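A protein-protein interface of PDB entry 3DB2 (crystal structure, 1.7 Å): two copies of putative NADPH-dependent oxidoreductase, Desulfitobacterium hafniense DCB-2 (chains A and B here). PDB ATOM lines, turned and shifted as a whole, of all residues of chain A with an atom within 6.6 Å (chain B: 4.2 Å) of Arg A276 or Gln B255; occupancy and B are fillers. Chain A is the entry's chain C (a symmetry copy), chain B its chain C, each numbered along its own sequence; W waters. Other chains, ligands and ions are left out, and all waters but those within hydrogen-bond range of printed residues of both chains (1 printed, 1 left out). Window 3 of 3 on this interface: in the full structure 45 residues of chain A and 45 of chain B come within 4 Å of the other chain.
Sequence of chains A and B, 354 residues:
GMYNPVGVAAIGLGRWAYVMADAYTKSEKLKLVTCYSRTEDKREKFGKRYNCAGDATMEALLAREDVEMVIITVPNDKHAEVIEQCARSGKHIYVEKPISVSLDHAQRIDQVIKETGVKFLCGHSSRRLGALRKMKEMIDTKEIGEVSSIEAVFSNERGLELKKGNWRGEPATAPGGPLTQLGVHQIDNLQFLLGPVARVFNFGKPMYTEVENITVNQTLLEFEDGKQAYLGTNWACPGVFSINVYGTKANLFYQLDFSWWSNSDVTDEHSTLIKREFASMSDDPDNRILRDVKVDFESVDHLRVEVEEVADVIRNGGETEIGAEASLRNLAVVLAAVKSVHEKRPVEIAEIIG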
ATOM      1  N   TYR A 246      24.933  -7.509   2.230  1.00  0.00           N
ATOM      2  CA  TYR A 246      24.340  -6.242   1.835  1.00  0.00           C
ATOM      3  C   TYR A 246      24.446  -5.272   3.017  1.00  0.00           C
ATOM      4  O   TYR A 246      23.888  -5.588   4.077  1.00  0.00           O
ATOM      5  CB  TYR A 246      22.877  -6.468   1.445  1.00  0.00           C
ATOM      6  CG  TYR A 246      22.812  -7.433   0.265  1.00  0.00           C
ATOM      7  CD1 TYR A 246      23.083  -6.986  -1.019  1.00  0.00           C
ATOM      8  CD2 TYR A 246      22.502  -8.781   0.424  1.00  0.00           C
ATOM      9  CE1 TYR A 246      23.031  -7.850  -2.096  1.00  0.00           C
ATOM     10  CE2 TYR A 246      22.451  -9.625  -0.676  1.00  0.00           C
ATOM     11  CZ  TYR A 246      22.715  -9.180  -1.942  1.00  0.00           C
ATOM     12  OH  TYR A 246      22.680 -10.017  -3.068  1.00  0.00           O
ATOM     13  N   LYS A 249      26.291   1.078   3.236  1.00  0.00           N
ATOM     14  CA  LYS A 249      27.302   1.795   2.490  1.00  0.00           C
ATOM     15  C   LYS A 249      27.922   0.978   1.357  1.00  0.00           C
ATOM     16  O   LYS A 249      28.483   1.517   0.415  1.00  0.00           O
ATOM     17  CB  LYS A 249      28.488   2.207   3.366  1.00  0.00           C
ATOM     18  CG  LYS A 249      28.240   3.071   4.581  1.00  0.00           C
ATOM     19  CD  LYS A 249      29.550   3.668   5.086  1.00  0.00           C
ATOM     20  CE  LYS A 249      30.088   3.032   6.339  1.00  0.00           C
ATOM     21  NZ  LYS A 249      29.442   3.449   7.614  1.00  0.00           N
ATOM     22  N   ALA A 250      27.863  -0.366   1.483  1.00  0.00           N
ATOM     23  CA  ALA A 250      28.575  -1.198   0.511  1.00  0.00           C
ATOM     24  C   ALA A 250      28.089  -2.652   0.566  1.00  0.00           C
ATOM     25  O   ALA A 250      27.698  -3.072   1.655  1.00  0.00           O
ATOM     26  CB  ALA A 250      30.075  -1.142   0.810  1.00  0.00           C
ATOM     27  N   ASN A 251      28.173  -3.343  -0.563  1.00  0.00           N
ATOM     28  CA  ASN A 251      27.887  -4.788  -0.560  1.00  0.00           C
ATOM     29  C   ASN A 251      29.168  -5.587  -0.792  1.00  0.00           C
ATOM     30  O   ASN A 251      30.051  -5.128  -1.499  1.00  0.00           O
ATOM     31  CB  ASN A 251      26.899  -5.105  -1.655  1.00  0.00           C
ATOM     32  CG  ASN A 251      25.573  -4.410  -1.500  1.00  0.00           C
ATOM     33  OD1 ASN A 251      25.085  -4.160  -0.421  1.00  0.00           O
ATOM     34  ND2 ASN A 251      24.964  -4.077  -2.643  1.00  0.00           N
ATOM     35  N   LEU A 252      29.241  -6.785  -0.229  1.00  0.00           N
ATOM     36  CA  LEU A 252      30.344  -7.693  -0.503  1.00  0.00           C
ATOM     37  C   LEU A 252      29.835  -8.939  -1.239  1.00  0.00           C
ATOM     38  O   LEU A 252      28.787  -9.477  -0.838  1.00  0.00           O
ATOM     39  CB  LEU A 252      30.982  -8.135   0.795  1.00  0.00           C
ATOM     40  CG  LEU A 252      31.426  -7.076   1.778  1.00  0.00           C
ATOM     41  CD1 LEU A 252      31.841  -7.711   3.091  1.00  0.00           C
ATOM     42  CD2 LEU A 252      32.553  -6.256   1.159  1.00  0.00           C
ATOM     43  N   PHE A 253      30.598  -9.352  -2.217  1.00  0.00           N
ATOM     44  CA  PHE A 253      30.317 -10.575  -2.984  1.00  0.00           C
ATOM     45  C   PHE A 253      31.551 -11.469  -2.962  1.00  0.00           C
ATOM     46  O   PHE A 253      32.583 -11.140  -3.523  1.00  0.00           O
ATOM     47  CB  PHE A 253      29.961 -10.275  -4.437  1.00  0.00           C
ATOM     48  CG  PHE A 253      28.865  -9.245  -4.613  1.00  0.00           C
ATOM     49  CD1 PHE A 253      27.575  -9.540  -4.214  1.00  0.00           C
ATOM     50  CD2 PHE A 253      29.158  -8.007  -5.180  1.00  0.00           C
ATOM     51  CE1 PHE A 253      26.571  -8.596  -4.391  1.00  0.00           C
ATOM     52  CE2 PHE A 253      28.151  -7.054  -5.338  1.00  0.00           C
ATOM     53  CZ  PHE A 253      26.879  -7.345  -4.905  1.00  0.00           C
ATOM     54  N   ILE A 274      34.592  -9.104  -3.681  1.00  0.00           N
ATOM     55  CA  ILE A 274      34.410  -7.832  -4.416  1.00  0.00           C
ATOM     56  C   ILE A 274      33.540  -6.961  -3.544  1.00  0.00           C
ATOM     57  O   ILE A 274      32.606  -7.451  -2.930  1.00  0.00           O
ATOM     58  CB  ILE A 274      33.847  -8.122  -5.805  1.00  0.00           C
ATOM     59  CG1 ILE A 274      34.921  -8.638  -6.797  1.00  0.00           C
ATOM     60  CG2 ILE A 274      33.091  -6.912  -6.328  1.00  0.00           C
ATOM     61  CD1 ILE A 274      35.579  -7.491  -7.552  1.00  0.00           C
ATOM     62  N   LYS A 275      33.871  -5.681  -3.441  1.00  0.00           N
ATOM     63  CA  LYS A 275      33.127  -4.659  -2.755  1.00  0.00           C
ATOM     64  C   LYS A 275      32.406  -3.765  -3.780  1.00  0.00           C
ATOM     65  O   LYS A 275      33.037  -3.229  -4.691  1.00  0.00           O
ATOM     66  CB  LYS A 275      34.031  -3.761  -1.916  1.00  0.00           C
ATOM     67  CG  LYS A 275      33.383  -2.813  -0.942  1.00  0.00           C
ATOM     68  CD  LYS A 275      34.399  -1.764  -0.455  1.00  0.00           C
ATOM     69  CE  LYS A 275      34.062  -1.255   0.940  1.00  0.00           C
ATOM     70  NZ  LYS A 275      34.921  -0.096   1.313  1.00  0.00           N
ATOM     71  N   ARG A 276      31.110  -3.626  -3.599  1.00  0.00           N
ATOM     72  CA  ARG A 276      30.306  -2.737  -4.436  1.00  0.00           C
ATOM     73  C   ARG A 276      29.957  -1.507  -3.606  1.00  0.00           C
ATOM     74  O   ARG A 276      29.283  -1.664  -2.580  1.00  0.00           O
ATOM     75  CB  ARG A 276      29.051  -3.425  -4.959  1.00  0.00           C
ATOM     76  CG  ARG A 276      28.148  -2.424  -5.714  1.00  0.00           C
ATOM     77  CD  ARG A 276      26.971  -3.174  -6.356  1.00  0.00           C
ATOM     78  NE  ARG A 276      27.545  -3.994  -7.430  1.00  0.00           N
ATOM     79  CZ  ARG A 276      26.790  -4.742  -8.233  1.00  0.00           C
ATOM     80  NH1 ARG A 276      25.474  -4.736  -8.047  1.00  0.00           N
ATOM     81  NH2 ARG A 276      27.376  -5.456  -9.185  1.00  0.00           N
ATOM     82  N   GLU A 277      30.417  -0.319  -4.014  1.00  0.00           N
ATOM     83  CA  GLU A 277      30.223   0.843  -3.146  1.00  0.00           C
ATOM     84  C   GLU A 277      29.878   2.061  -3.981  1.00  0.00           C
ATOM     85  O   GLU A 277      30.092   1.996  -5.189  1.00  0.00           O
ATOM     86  CB  GLU A 277      31.501   1.130  -2.344  1.00  0.00           C
ATOM     87  CG  GLU A 277      32.643   1.442  -3.292  1.00  0.00           C
ATOM     88  CD  GLU A 277      33.959   1.766  -2.643  1.00  0.00           C
ATOM     89  OE1 GLU A 277      33.987   1.836  -1.405  1.00  0.00           O
ATOM     90  OE2 GLU A 277      34.937   1.924  -3.404  1.00  0.00           O
ATOM     91  N   PHE A 278      29.374   3.111  -3.353  1.00  0.00           N
ATOM     92  CA  PHE A 278      29.109   4.352  -4.074  1.00  0.00           C
ATOM     93  C   PHE A 278      30.464   4.990  -4.375  1.00  0.00           C
ATOM     94  O   PHE A 278      31.296   5.001  -3.473  1.00  0.00           O
ATOM     95  CB  PHE A 278      28.223   5.311  -3.291  1.00  0.00           C
ATOM     96  CG  PHE A 278      26.912   4.704  -2.833  1.00  0.00           C
ATOM     97  CD1 PHE A 278      25.884   4.546  -3.754  1.00  0.00           C
ATOM     98  CD2 PHE A 278      26.740   4.299  -1.526  1.00  0.00           C
ATOM     99  CE1 PHE A 278      24.685   3.989  -3.350  1.00  0.00           C
ATOM    100  CE2 PHE A 278      25.537   3.754  -1.112  1.00  0.00           C
ATOM    101  CZ  PHE A 278      24.518   3.597  -2.038  1.00  0.00           C
ATOM    102  N   LEU A 290      28.003   3.688  -8.828  1.00  0.00           N
ATOM    103  CA  LEU A 290      28.580   2.563  -8.094  1.00  0.00           C
ATOM    104  C   LEU A 290      29.834   2.009  -8.762  1.00  0.00           C
ATOM    105  O   LEU A 290      29.962   1.955  -9.993  1.00  0.00           O
ATOM    106  CB  LEU A 290      27.513   1.477  -7.973  1.00  0.00           C
ATOM    107  CG  LEU A 290      26.279   1.768  -7.126  1.00  0.00           C
ATOM    108  CD1 LEU A 290      25.246   0.660  -7.300  1.00  0.00           C
ATOM    109  CD2 LEU A 290      26.662   1.930  -5.666  1.00  0.00           C
ATOM    110  N   ARG A 291      30.796   1.566  -7.952  1.00  0.00           N
ATOM    111  CA  ARG A 291      31.959   0.858  -8.468  1.00  0.00           C
ATOM    112  C   ARG A 291      32.153  -0.471  -7.718  1.00  0.00           C
ATOM    113  O   ARG A 291      31.860  -0.501  -6.525  1.00  0.00           O
ATOM    114  CB  ARG A 291      33.220   1.696  -8.361  1.00  0.00           C
ATOM    115  CG  ARG A 291      33.717   1.978  -6.962  1.00  0.00           C
ATOM    116  CD  ARG A 291      35.156   2.489  -6.981  1.00  0.00           C
ATOM    117  NE  ARG A 291      35.647   2.805  -5.649  1.00  0.00           N
ATOM    118  CZ  ARG A 291      35.852   3.977  -5.075  1.00  0.00           C
ATOM    119  NH1 ARG A 291      35.615   5.123  -5.695  1.00  0.00           N
ATOM    120  NH2 ARG A 291      36.314   4.032  -3.822  1.00  0.00           N
ATOM    121  N   ASP A 292      32.629  -1.447  -8.463  1.00  0.00           N
ATOM    122  CA  ASP A 292      33.006  -2.768  -7.955  1.00  0.00           C
ATOM    123  C   ASP A 292      34.526  -2.869  -7.844  1.00  0.00           C
ATOM    124  O   ASP A 292      35.238  -2.773  -8.845  1.00  0.00           O
ATOM    125  CB  ASP A 292      32.486  -3.908  -8.824  1.00  0.00           C
ATOM    126  CG  ASP A 292      30.993  -4.137  -8.712  1.00  0.00           C
ATOM    127  OD1 ASP A 292      30.364  -3.553  -7.805  1.00  0.00           O
ATOM    128  OD2 ASP A 292      30.429  -4.902  -9.525  1.00  0.00           O
ATOM    129  N   VAL A 293      35.024  -3.061  -6.633  1.00  0.00           N
ATOM    130  CA  VAL A 293      36.431  -3.081  -6.319  1.00  0.00           C
ATOM    131  C   VAL A 293      36.889  -4.428  -5.734  1.00  0.00           C
ATOM    132  O   VAL A 293      36.267  -4.951  -4.797  1.00  0.00           O
ATOM    133  CB  VAL A 293      36.817  -2.021  -5.265  1.00  0.00           C
ATOM    134  CG1 VAL A 293      38.340  -2.029  -5.150  1.00  0.00           C
ATOM    135  CG2 VAL A 293      36.312  -0.643  -5.631  1.00  0.00           C
ATOM    136  N   PRO B 238      23.373  -0.501  -1.648  1.00  0.00           N
ATOM    137  CA  PRO B 238      23.611  -0.170  -3.054  1.00  0.00           C
ATOM    138  C   PRO B 238      22.916  -1.116  -4.032  1.00  0.00           C
ATOM    139  O   PRO B 238      22.649  -2.279  -3.698  1.00  0.00           O
ATOM    140  CB  PRO B 238      25.115  -0.294  -3.192  1.00  0.00           C
ATOM    141  CG  PRO B 238      25.609   0.060  -1.821  1.00  0.00           C
ATOM    142  CD  PRO B 238      24.630  -0.624  -0.884  1.00  0.00           C
ATOM    143  N   GLY B 239      22.612  -0.593  -5.223  1.00  0.00           N
ATOM    144  CA  GLY B 239      21.800  -1.283  -6.200  1.00  0.00           C
ATOM    145  C   GLY B 239      22.371  -2.613  -6.677  1.00  0.00           C
ATOM    146  O   GLY B 239      23.547  -2.743  -7.032  1.00  0.00           O
ATOM    147  N   VAL B 240      21.513  -3.629  -6.695  1.00  0.00           N
ATOM    148  CA  VAL B 240      21.825  -4.957  -7.205  1.00  0.00           C
ATOM    149  C   VAL B 240      20.558  -5.454  -7.934  1.00  0.00           C
ATOM    150  O   VAL B 240      19.473  -5.267  -7.373  1.00  0.00           O
ATOM    151  CB  VAL B 240      22.152  -6.037  -6.167  1.00  0.00           C
ATOM    152  CG1 VAL B 240      22.392  -7.408  -6.821  1.00  0.00           C
ATOM    153  CG2 VAL B 240      23.337  -5.641  -5.310  1.00  0.00           C
ATOM    154  N   PHE B 241      20.771  -6.032  -9.101  1.00  0.00           N
ATOM    155  CA  PHE B 241      19.746  -6.760  -9.839  1.00  0.00           C
ATOM    156  C   PHE B 241      20.445  -8.036 -10.345  1.00  0.00           C
ATOM    157  O   PHE B 241      21.248  -7.936 -11.273  1.00  0.00           O
ATOM    158  CB  PHE B 241      19.121  -6.015 -10.992  1.00  0.00           C
ATOM    159  CG  PHE B 241      17.931  -6.617 -11.703  1.00  0.00           C
ATOM    160  CD1 PHE B 241      17.985  -7.780 -12.468  1.00  0.00           C
ATOM    161  CD2 PHE B 241      16.692  -5.991 -11.633  1.00  0.00           C
ATOM    162  CE1 PHE B 241      16.915  -8.344 -13.113  1.00  0.00           C
ATOM    163  CE2 PHE B 241      15.593  -6.550 -12.261  1.00  0.00           C
ATOM    164  CZ  PHE B 241      15.688  -7.712 -12.994  1.00  0.00           C
ATOM    165  N   SER B 242      20.054  -9.163  -9.752  1.00  0.00           N
ATOM    166  CA  SER B 242      20.694 -10.424 -10.142  1.00  0.00           C
ATOM    167  C   SER B 242      19.700 -11.579 -10.192  1.00  0.00           C
ATOM    168  O   SER B 242      18.662 -11.553  -9.554  1.00  0.00           O
ATOM    169  CB  SER B 242      21.831 -10.727  -9.174  1.00  0.00           C
ATOM    170  OG  SER B 242      21.385 -10.797  -7.841  1.00  0.00           O
ATOM    171  N   TYR B 254      23.406 -14.010 -13.727  1.00  0.00           N
ATOM    172  CA  TYR B 254      23.062 -12.771 -14.409  1.00  0.00           C
ATOM    173  C   TYR B 254      23.112 -11.602 -13.414  1.00  0.00           C
ATOM    174  O   TYR B 254      22.622 -11.745 -12.287  1.00  0.00           O
ATOM    175  CB  TYR B 254      21.675 -12.855 -15.007  1.00  0.00           C
ATOM    176  CG  TYR B 254      21.051 -11.623 -15.599  1.00  0.00           C
ATOM    177  CD1 TYR B 254      21.498 -11.108 -16.811  1.00  0.00           C
ATOM    178  CD2 TYR B 254      19.995 -10.959 -14.971  1.00  0.00           C
ATOM    179  CE1 TYR B 254      20.925  -9.976 -17.351  1.00  0.00           C
ATOM    180  CE2 TYR B 254      19.419  -9.824 -15.537  1.00  0.00           C
ATOM    181  CZ  TYR B 254      19.888  -9.333 -16.728  1.00  0.00           C
ATOM    182  OH  TYR B 254      19.349  -8.215 -17.335  1.00  0.00           O
ATOM    183  N   GLN B 255      23.697 -10.514 -13.861  1.00  0.00           N
ATOM    184  CA  GLN B 255      23.787  -9.238 -13.189  1.00  0.00           C
ATOM    185  C   GLN B 255      23.370  -8.109 -14.127  1.00  0.00           C
ATOM    186  O   GLN B 255      23.830  -8.093 -15.263  1.00  0.00           O
ATOM    187  CB  GLN B 255      25.222  -8.936 -12.713  1.00  0.00           C
ATOM    188  CG  GLN B 255      25.666  -9.633 -11.453  1.00  0.00           C
ATOM    189  CD  GLN B 255      25.206  -8.986 -10.165  1.00  0.00           C
ATOM    190  OE1 GLN B 255      24.693  -7.866 -10.147  1.00  0.00           O
ATOM    191  NE2 GLN B 255      25.367  -9.674  -9.031  1.00  0.00           N
ATOM    192  N   LEU B 256      22.536  -7.197 -13.668  1.00  0.00           N
ATOM    193  CA  LEU B 256      22.208  -6.011 -14.471  1.00  0.00           C
ATOM    194  C   LEU B 256      22.497  -4.724 -13.721  1.00  0.00           C
ATOM    195  O   LEU B 256      22.236  -4.680 -12.518  1.00  0.00           O
ATOM    196  CB  LEU B 256      20.743  -6.086 -14.867  1.00  0.00           C
ATOM    197  CG  LEU B 256      20.125  -4.845 -15.522  1.00  0.00           C
ATOM    198  CD1 LEU B 256      20.652  -4.754 -16.955  1.00  0.00           C
ATOM    199  CD2 LEU B 256      18.622  -4.947 -15.402  1.00  0.00           C
ATOM    200  N   SER B 271      24.710  -5.471 -18.796  1.00  0.00           N
ATOM    201  CA  SER B 271      24.424  -6.701 -18.040  1.00  0.00           C
ATOM    202  C   SER B 271      25.461  -7.749 -18.422  1.00  0.00           C
ATOM    203  O   SER B 271      26.143  -7.609 -19.435  1.00  0.00           O
ATOM    204  CB  SER B 271      22.999  -7.165 -18.304  1.00  0.00           C
ATOM    205  OG  SER B 271      22.814  -7.722 -19.593  1.00  0.00           O
ATOM    206  N   THR B 272      25.581  -8.805 -17.632  1.00  0.00           N
ATOM    207  CA  THR B 272      26.507  -9.882 -17.894  1.00  0.00           C
ATOM    208  C   THR B 272      25.730 -11.188 -17.579  1.00  0.00           C
ATOM    209  O   THR B 272      25.016 -11.182 -16.569  1.00  0.00           O
ATOM    210  CB  THR B 272      27.758 -10.005 -17.027  1.00  0.00           C
ATOM    211  OG1 THR B 272      27.422  -9.589 -15.688  1.00  0.00           O
ATOM    212  CG2 THR B 272      28.903  -9.147 -17.530  1.00  0.00           C
HETATM  213  O   HOH W   1      23.278 -10.732  -5.936  1.00  0.00           O
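No position is printed for both chains.
Of the 10 printed residues of chain B, 4 touch a printed residue of chain A.
Hydrophobic or aromatic side chains of chain B that line the printed part of chain A: Pro B238 and Val B240.
Among the printed residues, 12 pairs touch across the chains.
Among the printed residues, no Asp or Glu carboxylate lies within 4 Å of a Lys or Arg side-chain nitrogen of the other chain.
Water W1 lies within hydrogen-bond range of the side-chain hydroxyl of Ser B242 (2.7 Å) and the side-chain hydroxyl of Tyr A246 (3.0 Å).
ND2 of Asn A251 lies within hydrogen-bond range of O of Pro B238 (3.1 Å).
The guanidinium group (NH1) of Arg A276 lies within hydrogen-bond range of the backbone carbonyl oxygen (O) of Gly B239 (3.0 Å).
Of the printed residues of chain B, Lys A249 touches Pro B238 (3.9 Å).
Of chain B, only Gly B239, Val B240 and Gln B255 come within 4 Å of Arg A276.
Of the printed residues of chain B, Leu A290 touches Pro B238 and Gly B239.
Of the printed residues of chain A, Val B240 touches Tyr A246, Asn A251, Phe A253 and Arg A276.
Of chain A, only Arg A276 (3.7 Å) comes within 4 Å of Gln B255.
The nearest residue of chain B that does not touch Arg A276 is Pro B238 (4.1 Å).
Among the printed residues, merely in contact across the chains: Tyr A246 with Val B240, Lys A249 with Pro B238, Ala A250 with Pro B238, Asn A251 with Val B240, Phe A253 with Val B240, Arg A276 with Val B240, Arg A276 with Gln B255, Phe A278 with Pro B238, Leu A290 with Pro B238 and Leu A290 with Gly B239.
The backbone carbonyl oxygen (O) of Gln B255 sits at hydrogen-bond distance from the backbone NH (N) of Thr B272.
The backbone carbonyl oxygen (O) of Asn A251 sits at hydrogen-bond distance from the backbone NH (N) of Arg A276, 2.8 Å away.
The backbone NH (N) of Phe A253 sits at hydrogen-bond distance from the backbone carbonyl oxygen (O) of Ile A274 (2.9 Å).
OD1 of Asp A292 lies within salt-bridge range of NE of Arg A276 (2.9 Å).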
